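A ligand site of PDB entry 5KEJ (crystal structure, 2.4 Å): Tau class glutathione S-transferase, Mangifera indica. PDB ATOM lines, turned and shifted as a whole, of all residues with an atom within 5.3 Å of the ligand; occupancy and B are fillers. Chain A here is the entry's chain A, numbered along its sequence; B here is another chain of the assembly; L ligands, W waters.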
ATOM      1  N   PRO A  13      12.817  -6.480  18.130  1.00  0.00           N
ATOM      2  CA  PRO A  13      12.338  -7.481  19.098  1.00  0.00           C
ATOM      3  C   PRO A  13      12.255  -8.920  18.574  1.00  0.00           C
ATOM      4  O   PRO A  13      11.940  -9.828  19.355  1.00  0.00           O
ATOM      5  CB  PRO A  13      10.912  -6.993  19.435  1.00  0.00           C
ATOM      6  CG  PRO A  13      10.684  -5.740  18.673  1.00  0.00           C
ATOM      7  CD  PRO A  13      11.686  -5.704  17.575  1.00  0.00           C
ATOM      8  N   SER A  14      12.510  -9.126  17.293  1.00  0.00           N
ATOM      9  CA  SER A  14      12.263 -10.423  16.656  1.00  0.00           C
ATOM     10  C   SER A  14      13.395 -11.426  16.884  1.00  0.00           C
ATOM     11  O   SER A  14      14.529 -11.203  16.432  1.00  0.00           O
ATOM     12  CB  SER A  14      12.049 -10.244  15.161  1.00  0.00           C
ATOM     13  OG  SER A  14      11.915 -11.501  14.533  1.00  0.00           O
ATOM     14  N   PRO A  15      13.102 -12.551  17.549  1.00  0.00           N
ATOM     15  CA  PRO A  15      14.095 -13.627  17.741  1.00  0.00           C
ATOM     16  C   PRO A  15      14.605 -14.161  16.411  1.00  0.00           C
ATOM     17  O   PRO A  15      15.809 -14.428  16.282  1.00  0.00           O
ATOM     18  CB  PRO A  15      13.305 -14.699  18.504  1.00  0.00           C
ATOM     19  CG  PRO A  15      11.856 -14.369  18.254  1.00  0.00           C
ATOM     20  CD  PRO A  15      11.795 -12.883  18.144  1.00  0.00           C
ATOM     21  N   TYR A  16      13.718 -14.280  15.423  1.00  0.00           N
ATOM     22  CA  TYR A  16      14.090 -14.773  14.088  1.00  0.00           C
ATOM     23  C   TYR A  16      15.082 -13.864  13.391  1.00  0.00           C
ATOM     24  O   TYR A  16      16.030 -14.337  12.766  1.00  0.00           O
ATOM     25  CB  TYR A  16      12.837 -14.952  13.231  1.00  0.00           C
ATOM     26  CG  TYR A  16      11.981 -16.037  13.806  1.00  0.00           C
ATOM     27  CD1 TYR A  16      12.383 -17.355  13.726  1.00  0.00           C
ATOM     28  CD2 TYR A  16      10.789 -15.754  14.467  1.00  0.00           C
ATOM     29  CE1 TYR A  16      11.633 -18.372  14.284  1.00  0.00           C
ATOM     30  CE2 TYR A  16      10.015 -16.765  15.022  1.00  0.00           C
ATOM     31  CZ  TYR A  16      10.453 -18.082  14.918  1.00  0.00           C
ATOM     32  OH  TYR A  16       9.735 -19.115  15.449  1.00  0.00           O
ATOM     33  N   ARG A  19      18.613 -14.145  14.888  1.00  0.00           N
ATOM     34  CA  ARG A  19      19.417 -15.226  14.301  1.00  0.00           C
ATOM     35  C   ARG A  19      20.313 -14.751  13.193  1.00  0.00           C
ATOM     36  O   ARG A  19      21.464 -15.187  13.094  1.00  0.00           O
ATOM     37  CB  ARG A  19      18.519 -16.327  13.735  1.00  0.00           C
ATOM     38  CG  ARG A  19      17.854 -17.193  14.765  1.00  0.00           C
ATOM     39  CD  ARG A  19      16.866 -18.160  14.129  1.00  0.00           C
ATOM     40  NE  ARG A  19      16.393 -19.128  15.115  1.00  0.00           N
ATOM     41  CZ  ARG A  19      15.408 -19.994  14.909  1.00  0.00           C
ATOM     42  NH1 ARG A  19      15.056 -20.855  15.882  1.00  0.00           N
ATOM     43  NH2 ARG A  19      14.769 -20.015  13.742  1.00  0.00           N
ATOM     44  N   LEU A  38       5.383  -2.039  13.445  1.00  0.00           N
ATOM     45  CA  LEU A  38       4.118  -2.725  13.658  1.00  0.00           C
ATOM     46  C   LEU A  38       2.994  -2.081  12.843  1.00  0.00           C
ATOM     47  O   LEU A  38       2.789  -0.878  12.879  1.00  0.00           O
ATOM     48  CB  LEU A  38       3.746  -2.706  15.146  1.00  0.00           C
ATOM     49  CG  LEU A  38       3.424  -4.015  15.863  1.00  0.00           C
ATOM     50  CD1 LEU A  38       4.385  -5.122  15.471  1.00  0.00           C
ATOM     51  CD2 LEU A  38       3.484  -3.775  17.354  1.00  0.00           C
ATOM     52  N   LYS A  41       3.978  -2.634   6.166  1.00  0.00           N
ATOM     53  CA  LYS A  41       5.049  -3.384   5.495  1.00  0.00           C
ATOM     54  C   LYS A  41       5.862  -2.466   4.579  1.00  0.00           C
ATOM     55  O   LYS A  41       5.285  -1.781   3.722  1.00  0.00           O
ATOM     56  CB  LYS A  41       4.463  -4.542   4.688  1.00  0.00           C
ATOM     57  CG  LYS A  41       3.591  -5.489   5.502  1.00  0.00           C
ATOM     58  CD  LYS A  41       4.390  -6.639   6.102  1.00  0.00           C
ATOM     59  CE  LYS A  41       3.537  -7.439   7.109  1.00  0.00           C
ATOM     60  NZ  LYS A  41       3.216  -6.581   8.310  1.00  0.00           N
ATOM     61  N   HIS A  52       5.821 -14.696   1.655  1.00  0.00           N
ATOM     62  CA  HIS A  52       5.471 -14.705   3.078  1.00  0.00           C
ATOM     63  C   HIS A  52       5.280 -13.307   3.653  1.00  0.00           C
ATOM     64  O   HIS A  52       4.541 -13.142   4.619  1.00  0.00           O
ATOM     65  CB  HIS A  52       6.553 -15.404   3.891  1.00  0.00           C
ATOM     66  CG  HIS A  52       6.684 -16.868   3.618  1.00  0.00           C
ATOM     67  ND1 HIS A  52       5.632 -17.744   3.746  1.00  0.00           N
ATOM     68  CD2 HIS A  52       7.754 -17.614   3.247  1.00  0.00           C
ATOM     69  CE1 HIS A  52       6.037 -18.968   3.453  1.00  0.00           C
ATOM     70  NE2 HIS A  52       7.320 -18.918   3.145  1.00  0.00           N
ATOM     71  N   LYS A  53       5.974 -12.329   3.072  1.00  0.00           N
ATOM     72  CA  LYS A  53       6.055 -10.978   3.638  1.00  0.00           C
ATOM     73  C   LYS A  53       6.479 -10.996   5.106  1.00  0.00           C
ATOM     74  O   LYS A  53       5.922 -10.272   5.925  1.00  0.00           O
ATOM     75  CB  LYS A  53       4.722 -10.247   3.464  1.00  0.00           C
ATOM     76  CG  LYS A  53       4.233 -10.232   1.996  1.00  0.00           C
ATOM     77  CD  LYS A  53       2.858  -9.598   1.865  1.00  0.00           C
ATOM     78  CE  LYS A  53       1.844 -10.570   1.276  1.00  0.00           C
ATOM     79  NZ  LYS A  53       1.583 -11.789   2.129  1.00  0.00           N
ATOM     80  N   LYS A  54       7.475 -11.814   5.435  1.00  0.00           N
ATOM     81  CA  LYS A  54       7.994 -11.890   6.801  1.00  0.00           C
ATOM     82  C   LYS A  54       9.448 -11.450   6.895  1.00  0.00           C
ATOM     83  O   LYS A  54      10.197 -11.472   5.900  1.00  0.00           O
ATOM     84  CB  LYS A  54       7.861 -13.304   7.352  1.00  0.00           C
ATOM     85  CG  LYS A  54       6.444 -13.849   7.446  1.00  0.00           C
ATOM     86  CD  LYS A  54       6.462 -15.290   7.940  1.00  0.00           C
ATOM     87  CE  LYS A  54       5.093 -15.940   7.866  1.00  0.00           C
ATOM     88  NZ  LYS A  54       5.211 -17.406   8.126  1.00  0.00           N
ATOM     89  N   ILE A  55       9.856 -11.075   8.102  1.00  0.00           N
ATOM     90  CA  ILE A  55      11.267 -10.807   8.384  1.00  0.00           C
ATOM     91  C   ILE A  55      11.777 -11.959   9.244  1.00  0.00           C
ATOM     92  O   ILE A  55      10.990 -12.596   9.929  1.00  0.00           O
ATOM     93  CB  ILE A  55      11.438  -9.461   9.095  1.00  0.00           C
ATOM     94  CG1 ILE A  55      10.461  -9.405  10.282  1.00  0.00           C
ATOM     95  CG2 ILE A  55      11.202  -8.318   8.116  1.00  0.00           C
ATOM     96  CD1 ILE A  55      10.352  -8.076  10.939  1.00  0.00           C
ATOM     97  N   PRO A  56      13.091 -12.237   9.219  1.00  0.00           N
ATOM     98  CA  PRO A  56      14.130 -11.506   8.484  1.00  0.00           C
ATOM     99  C   PRO A  56      14.154 -11.819   6.996  1.00  0.00           C
ATOM    100  O   PRO A  56      13.658 -12.843   6.525  1.00  0.00           O
ATOM    101  CB  PRO A  56      15.422 -11.995   9.131  1.00  0.00           C
ATOM    102  CG  PRO A  56      15.094 -13.470   9.470  1.00  0.00           C
ATOM    103  CD  PRO A  56      13.644 -13.411   9.925  1.00  0.00           C
ATOM    104  N   GLU A  67      13.536 -16.635   5.334  1.00  0.00           N
ATOM    105  CA  GLU A  67      13.504 -17.701   6.354  1.00  0.00           C
ATOM    106  C   GLU A  67      14.834 -17.755   7.135  1.00  0.00           C
ATOM    107  O   GLU A  67      15.888 -18.009   6.576  1.00  0.00           O
ATOM    108  CB  GLU A  67      13.174 -19.073   5.751  1.00  0.00           C
ATOM    109  CG  GLU A  67      11.781 -19.150   5.101  1.00  0.00           C
ATOM    110  CD  GLU A  67      10.641 -19.174   6.134  1.00  0.00           C
ATOM    111  OE1 GLU A  67       9.681 -18.378   5.993  1.00  0.00           O
ATOM    112  OE2 GLU A  67      10.703 -19.997   7.086  1.00  0.00           O
ATOM    113  N   SER A  68      14.730 -17.501   8.438  1.00  0.00           N
ATOM    114  CA  SER A  68      15.880 -17.289   9.314  1.00  0.00           C
ATOM    115  C   SER A  68      16.938 -18.382   9.262  1.00  0.00           C
ATOM    116  O   SER A  68      18.131 -18.078   9.144  1.00  0.00           O
ATOM    117  CB  SER A  68      15.405 -17.114  10.760  1.00  0.00           C
ATOM    118  OG  SER A  68      14.642 -18.216  11.202  1.00  0.00           O
ATOM    119  N   LEU A  69      16.529 -19.643   9.317  1.00  0.00           N
ATOM    120  CA  LEU A  69      17.493 -20.745   9.268  1.00  0.00           C
ATOM    121  C   LEU A  69      18.095 -20.953   7.869  1.00  0.00           C
ATOM    122  O   LEU A  69      19.242 -21.390   7.726  1.00  0.00           O
ATOM    123  CB  LEU A  69      16.842 -22.033   9.778  1.00  0.00           C
ATOM    124  CG  LEU A  69      16.344 -22.014  11.230  1.00  0.00           C
ATOM    125  CD1 LEU A  69      15.775 -23.369  11.601  1.00  0.00           C
ATOM    126  CD2 LEU A  69      17.476 -21.628  12.176  1.00  0.00           C
ATOM    127  N   ASP A 104      11.632 -24.557  16.460  1.00  0.00           N
ATOM    128  CA  ASP A 104      10.659 -23.776  15.716  1.00  0.00           C
ATOM    129  C   ASP A 104       9.313 -24.491  15.596  1.00  0.00           C
ATOM    130  O   ASP A 104       8.276 -23.848  15.598  1.00  0.00           O
ATOM    131  CB  ASP A 104      11.198 -23.427  14.342  1.00  0.00           C
ATOM    132  CG  ASP A 104      12.328 -22.387  14.408  1.00  0.00           C
ATOM    133  OD1 ASP A 104      12.607 -21.908  15.523  1.00  0.00           O
ATOM    134  OD2 ASP A 104      12.915 -22.060  13.367  1.00  0.00           O
ATOM    135  N   TYR A 108       9.037 -23.303  20.721  1.00  0.00           N
ATOM    136  CA  TYR A 108       8.621 -21.896  20.722  1.00  0.00           C
ATOM    137  C   TYR A 108       7.106 -21.722  20.623  1.00  0.00           C
ATOM    138  O   TYR A 108       6.572 -20.884  21.333  1.00  0.00           O
ATOM    139  CB  TYR A 108       9.295 -21.122  19.593  1.00  0.00           C
ATOM    140  CG  TYR A 108       9.122 -19.631  19.713  1.00  0.00           C
ATOM    141  CD1 TYR A 108       9.554 -18.950  20.848  1.00  0.00           C
ATOM    142  CD2 TYR A 108       8.554 -18.882  18.684  1.00  0.00           C
ATOM    143  CE1 TYR A 108       9.415 -17.568  20.964  1.00  0.00           C
ATOM    144  CE2 TYR A 108       8.417 -17.498  18.786  1.00  0.00           C
ATOM    145  CZ  TYR A 108       8.848 -16.841  19.926  1.00  0.00           C
ATOM    146  OH  TYR A 108       8.705 -15.467  20.019  1.00  0.00           O
ATOM    147  N   TRP A 169      12.820 -13.516  24.898  1.00  0.00           N
ATOM    148  CA  TRP A 169      11.387 -13.778  25.042  1.00  0.00           C
ATOM    149  C   TRP A 169      11.104 -14.837  26.113  1.00  0.00           C
ATOM    150  O   TRP A 169      10.039 -14.813  26.730  1.00  0.00           O
ATOM    151  CB  TRP A 169      10.782 -14.210  23.702  1.00  0.00           C
ATOM    152  CG  TRP A 169      10.437 -13.034  22.848  1.00  0.00           C
ATOM    153  CD1 TRP A 169      11.119 -12.581  21.764  1.00  0.00           C
ATOM    154  CD2 TRP A 169       9.356 -12.125  23.053  1.00  0.00           C
ATOM    155  NE1 TRP A 169      10.520 -11.448  21.264  1.00  0.00           N
ATOM    156  CE2 TRP A 169       9.435 -11.147  22.045  1.00  0.00           C
ATOM    157  CE3 TRP A 169       8.325 -12.037  23.994  1.00  0.00           C
ATOM    158  CZ2 TRP A 169       8.522 -10.110  21.936  1.00  0.00           C
ATOM    159  CZ3 TRP A 169       7.414 -11.006  23.892  1.00  0.00           C
ATOM    160  CH2 TRP A 169       7.518 -10.055  22.863  1.00  0.00           C
ATOM    161  N   PHE A 216       7.806  -3.687  24.934  1.00  0.00           N
ATOM    162  CA  PHE A 216       7.339  -3.859  23.560  1.00  0.00           C
ATOM    163  C   PHE A 216       6.310  -4.973  23.535  1.00  0.00           C
ATOM    164  O   PHE A 216       5.366  -4.947  22.745  1.00  0.00           O
ATOM    165  CB  PHE A 216       8.483  -4.182  22.591  1.00  0.00           C
ATOM    166  CG  PHE A 216       7.995  -4.804  21.297  1.00  0.00           C
ATOM    167  CD1 PHE A 216       7.563  -4.005  20.252  1.00  0.00           C
ATOM    168  CD2 PHE A 216       7.920  -6.184  21.144  1.00  0.00           C
ATOM    169  CE1 PHE A 216       7.084  -4.558  19.073  1.00  0.00           C
ATOM    170  CE2 PHE A 216       7.436  -6.756  19.976  1.00  0.00           C
ATOM    171  CZ  PHE A 216       7.019  -5.941  18.927  1.00  0.00           C
ATOM    172  N   LEU A 220       2.623  -4.587  21.987  1.00  0.00           N
ATOM    173  CA  LEU A 220       1.941  -5.523  21.116  1.00  0.00           C
ATOM    174  C   LEU A 220       0.608  -5.982  21.734  1.00  0.00           C
ATOM    175  O   LEU A 220      -0.006  -6.935  21.269  1.00  0.00           O
ATOM    176  CB  LEU A 220       2.859  -6.713  20.812  1.00  0.00           C
ATOM    177  CG  LEU A 220       2.487  -7.699  19.694  1.00  0.00           C
ATOM    178  CD1 LEU A 220       2.071  -7.006  18.399  1.00  0.00           C
ATOM    179  CD2 LEU A 220       3.642  -8.667  19.450  1.00  0.00           C
ATOM    180  N   GLU B 105       5.340 -26.335   4.815  1.00  0.00           N
ATOM    181  CA  GLU B 105       4.661 -25.404   5.724  1.00  0.00           C
ATOM    182  C   GLU B 105       3.266 -25.042   5.240  1.00  0.00           C
ATOM    183  O   GLU B 105       2.339 -24.944   6.043  1.00  0.00           O
ATOM    184  CB  GLU B 105       5.484 -24.122   5.911  1.00  0.00           C
ATOM    185  CG  GLU B 105       5.084 -23.292   7.136  1.00  0.00           C
ATOM    186  CD  GLU B 105       5.634 -21.857   7.119  1.00  0.00           C
ATOM    187  OE1 GLU B 105       6.716 -21.621   6.533  1.00  0.00           O
ATOM    188  OE2 GLU B 105       4.970 -20.945   7.678  1.00  0.00           O
HETATM  189  N1  LIG L   1       9.533 -18.686   9.556  1.00  0.00           N
HETATM  190  C1  LIG L   1      10.158 -17.379   9.681  1.00  0.00           C
HETATM  191  C2  LIG L   1      11.616 -17.565   9.901  1.00  0.00           C
HETATM  192  O1  LIG L   1      12.375 -16.867   9.303  1.00  0.00           O
HETATM  193  O2  LIG L   1      12.021 -18.428  10.652  1.00  0.00           O
HETATM  194  C3  LIG L   1       9.523 -16.583  10.819  1.00  0.00           C
HETATM  195  C4  LIG L   1       9.169 -15.173  10.391  1.00  0.00           C
HETATM  196  C5  LIG L   1       8.414 -14.433  11.461  1.00  0.00           C
HETATM  197  O3  LIG L   1       7.452 -14.914  11.933  1.00  0.00           O
HETATM  198  N2  LIG L   1       8.874 -13.276  11.875  1.00  0.00           N
HETATM  199  C6  LIG L   1       8.101 -12.422  12.745  1.00  0.00           C
HETATM  200  C7  LIG L   1       7.308 -11.454  11.952  1.00  0.00           C
HETATM  201  O4  LIG L   1       6.840 -10.473  12.468  1.00  0.00           O
HETATM  202  C8  LIG L   1       8.972 -11.601  13.692  1.00  0.00           C
HETATM  203  S1  LIG L   1       9.455 -12.396  15.200  1.00  0.00           S
HETATM  204  C9  LIG L   1       8.037 -13.273  15.730  1.00  0.00           C
HETATM  205  C10 LIG L   1       7.915 -13.235  17.254  1.00  0.00           C
HETATM  206  C11 LIG L   1       7.107 -12.027  17.722  1.00  0.00           C
HETATM  207  C12 LIG L   1       7.988 -10.851  18.121  1.00  0.00           C
HETATM  208  C13 LIG L   1       8.116  -9.766  17.064  1.00  0.00           C
HETATM  209  C14 LIG L   1       6.858  -9.566  16.267  1.00  0.00           C
HETATM  210  N3  LIG L   1       7.173 -11.727  10.685  1.00  0.00           N
HETATM  211  C15 LIG L   1       6.345 -10.941   9.830  1.00  0.00           C
HETATM  212  C16 LIG L   1       4.971 -11.521   9.890  1.00  0.00           C
HETATM  213  O5  LIG L   1       4.149 -11.254   8.991  1.00  0.00           O
HETATM  214  O6  LIG L   1       4.726 -12.245  10.858  1.00  0.00           O
HETATM  215  O   HOH W   1      11.840 -14.855   7.135  1.00  0.00           O
HETATM  216  O   HOH W   2      10.180 -20.562  12.056  1.00  0.00           O
HETATM  217  O   HOH W   3      13.641 -20.648   9.269  1.00  0.00           O
HETATM  218  O   HOH W   4       5.799 -14.898  16.232  1.00  0.00           O
HETATM  219  O   HOH W   5       6.914 -19.982  10.072  1.00  0.00           O
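Water W5 lies within hydrogen-bond range of a nitrogen (N1) of the ligand (3.0 Å) and the side-chain carboxylate (OE2) of Glu 105 of chain B (3.2 Å). Water W1 lies within hydrogen-bond range of O of Pro 56 (2.8 Å), O1 of the ligand (3.0 Å) and N of Glu 67 (3.0 Å). Water W3 lies within hydrogen-bond range of the backbone NH of Leu 69, an oxygen (O2) of the ligand and the side-chain hydroxyl of Ser 68. Water W2 bridges an oxygen (O2) of the ligand (3.1 Å) and the side-chain carboxylate (OD2) of Asp 104 (3.4 Å).
O of Pro 13 is in hydrogen-bond range of NE1 of Trp 169 (2.9 Å). The guanidinium group of Arg 19 is in hydrogen-bond range of the side-chain hydroxyl of Ser 68, at 3.1 Å. NZ of Lys 54 lies within salt-bridge range of OE2 of Glu 105 of chain B (3.6 Å). N of Tyr 16 lies close to OG of Ser 14 (3.4 Å).
The side-chain hydroxyl of Ser 14 sits close to a sulfur (S1) of the ligand (2.7 Å). The side-chain hydroxyl (OG) of Ser 68 lies within hydrogen-bond range of an oxygen (O2) of the ligand. N of Ser 68 lies within hydrogen-bond range of O1 of the ligand (2.6 Å). OE2 of Glu 67 lies within salt-bridge range of N1 of the ligand. N2 of the ligand is in hydrogen-bond range of O of Ile 55.
Pro 15 touches the ligand (CD to S1, 3.8 Å). CD1 of Tyr 16 touches O2 of the ligand, 3.3 Å away. O of Lys 53 touches O5 of the ligand, at 3.7 Å. Lys 54 touches the ligand. Pro 56 touches the ligand. Tyr 108 touches the ligand. Trp 169 touches the ligand. Hydrophobic or aromatic side chains within 4 Å of the ligand: Pro 15, Tyr 16, Pro 56 and Trp 169. The nearest printed residue that does not touch the ligand is Phe 216 (4.2 Å).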
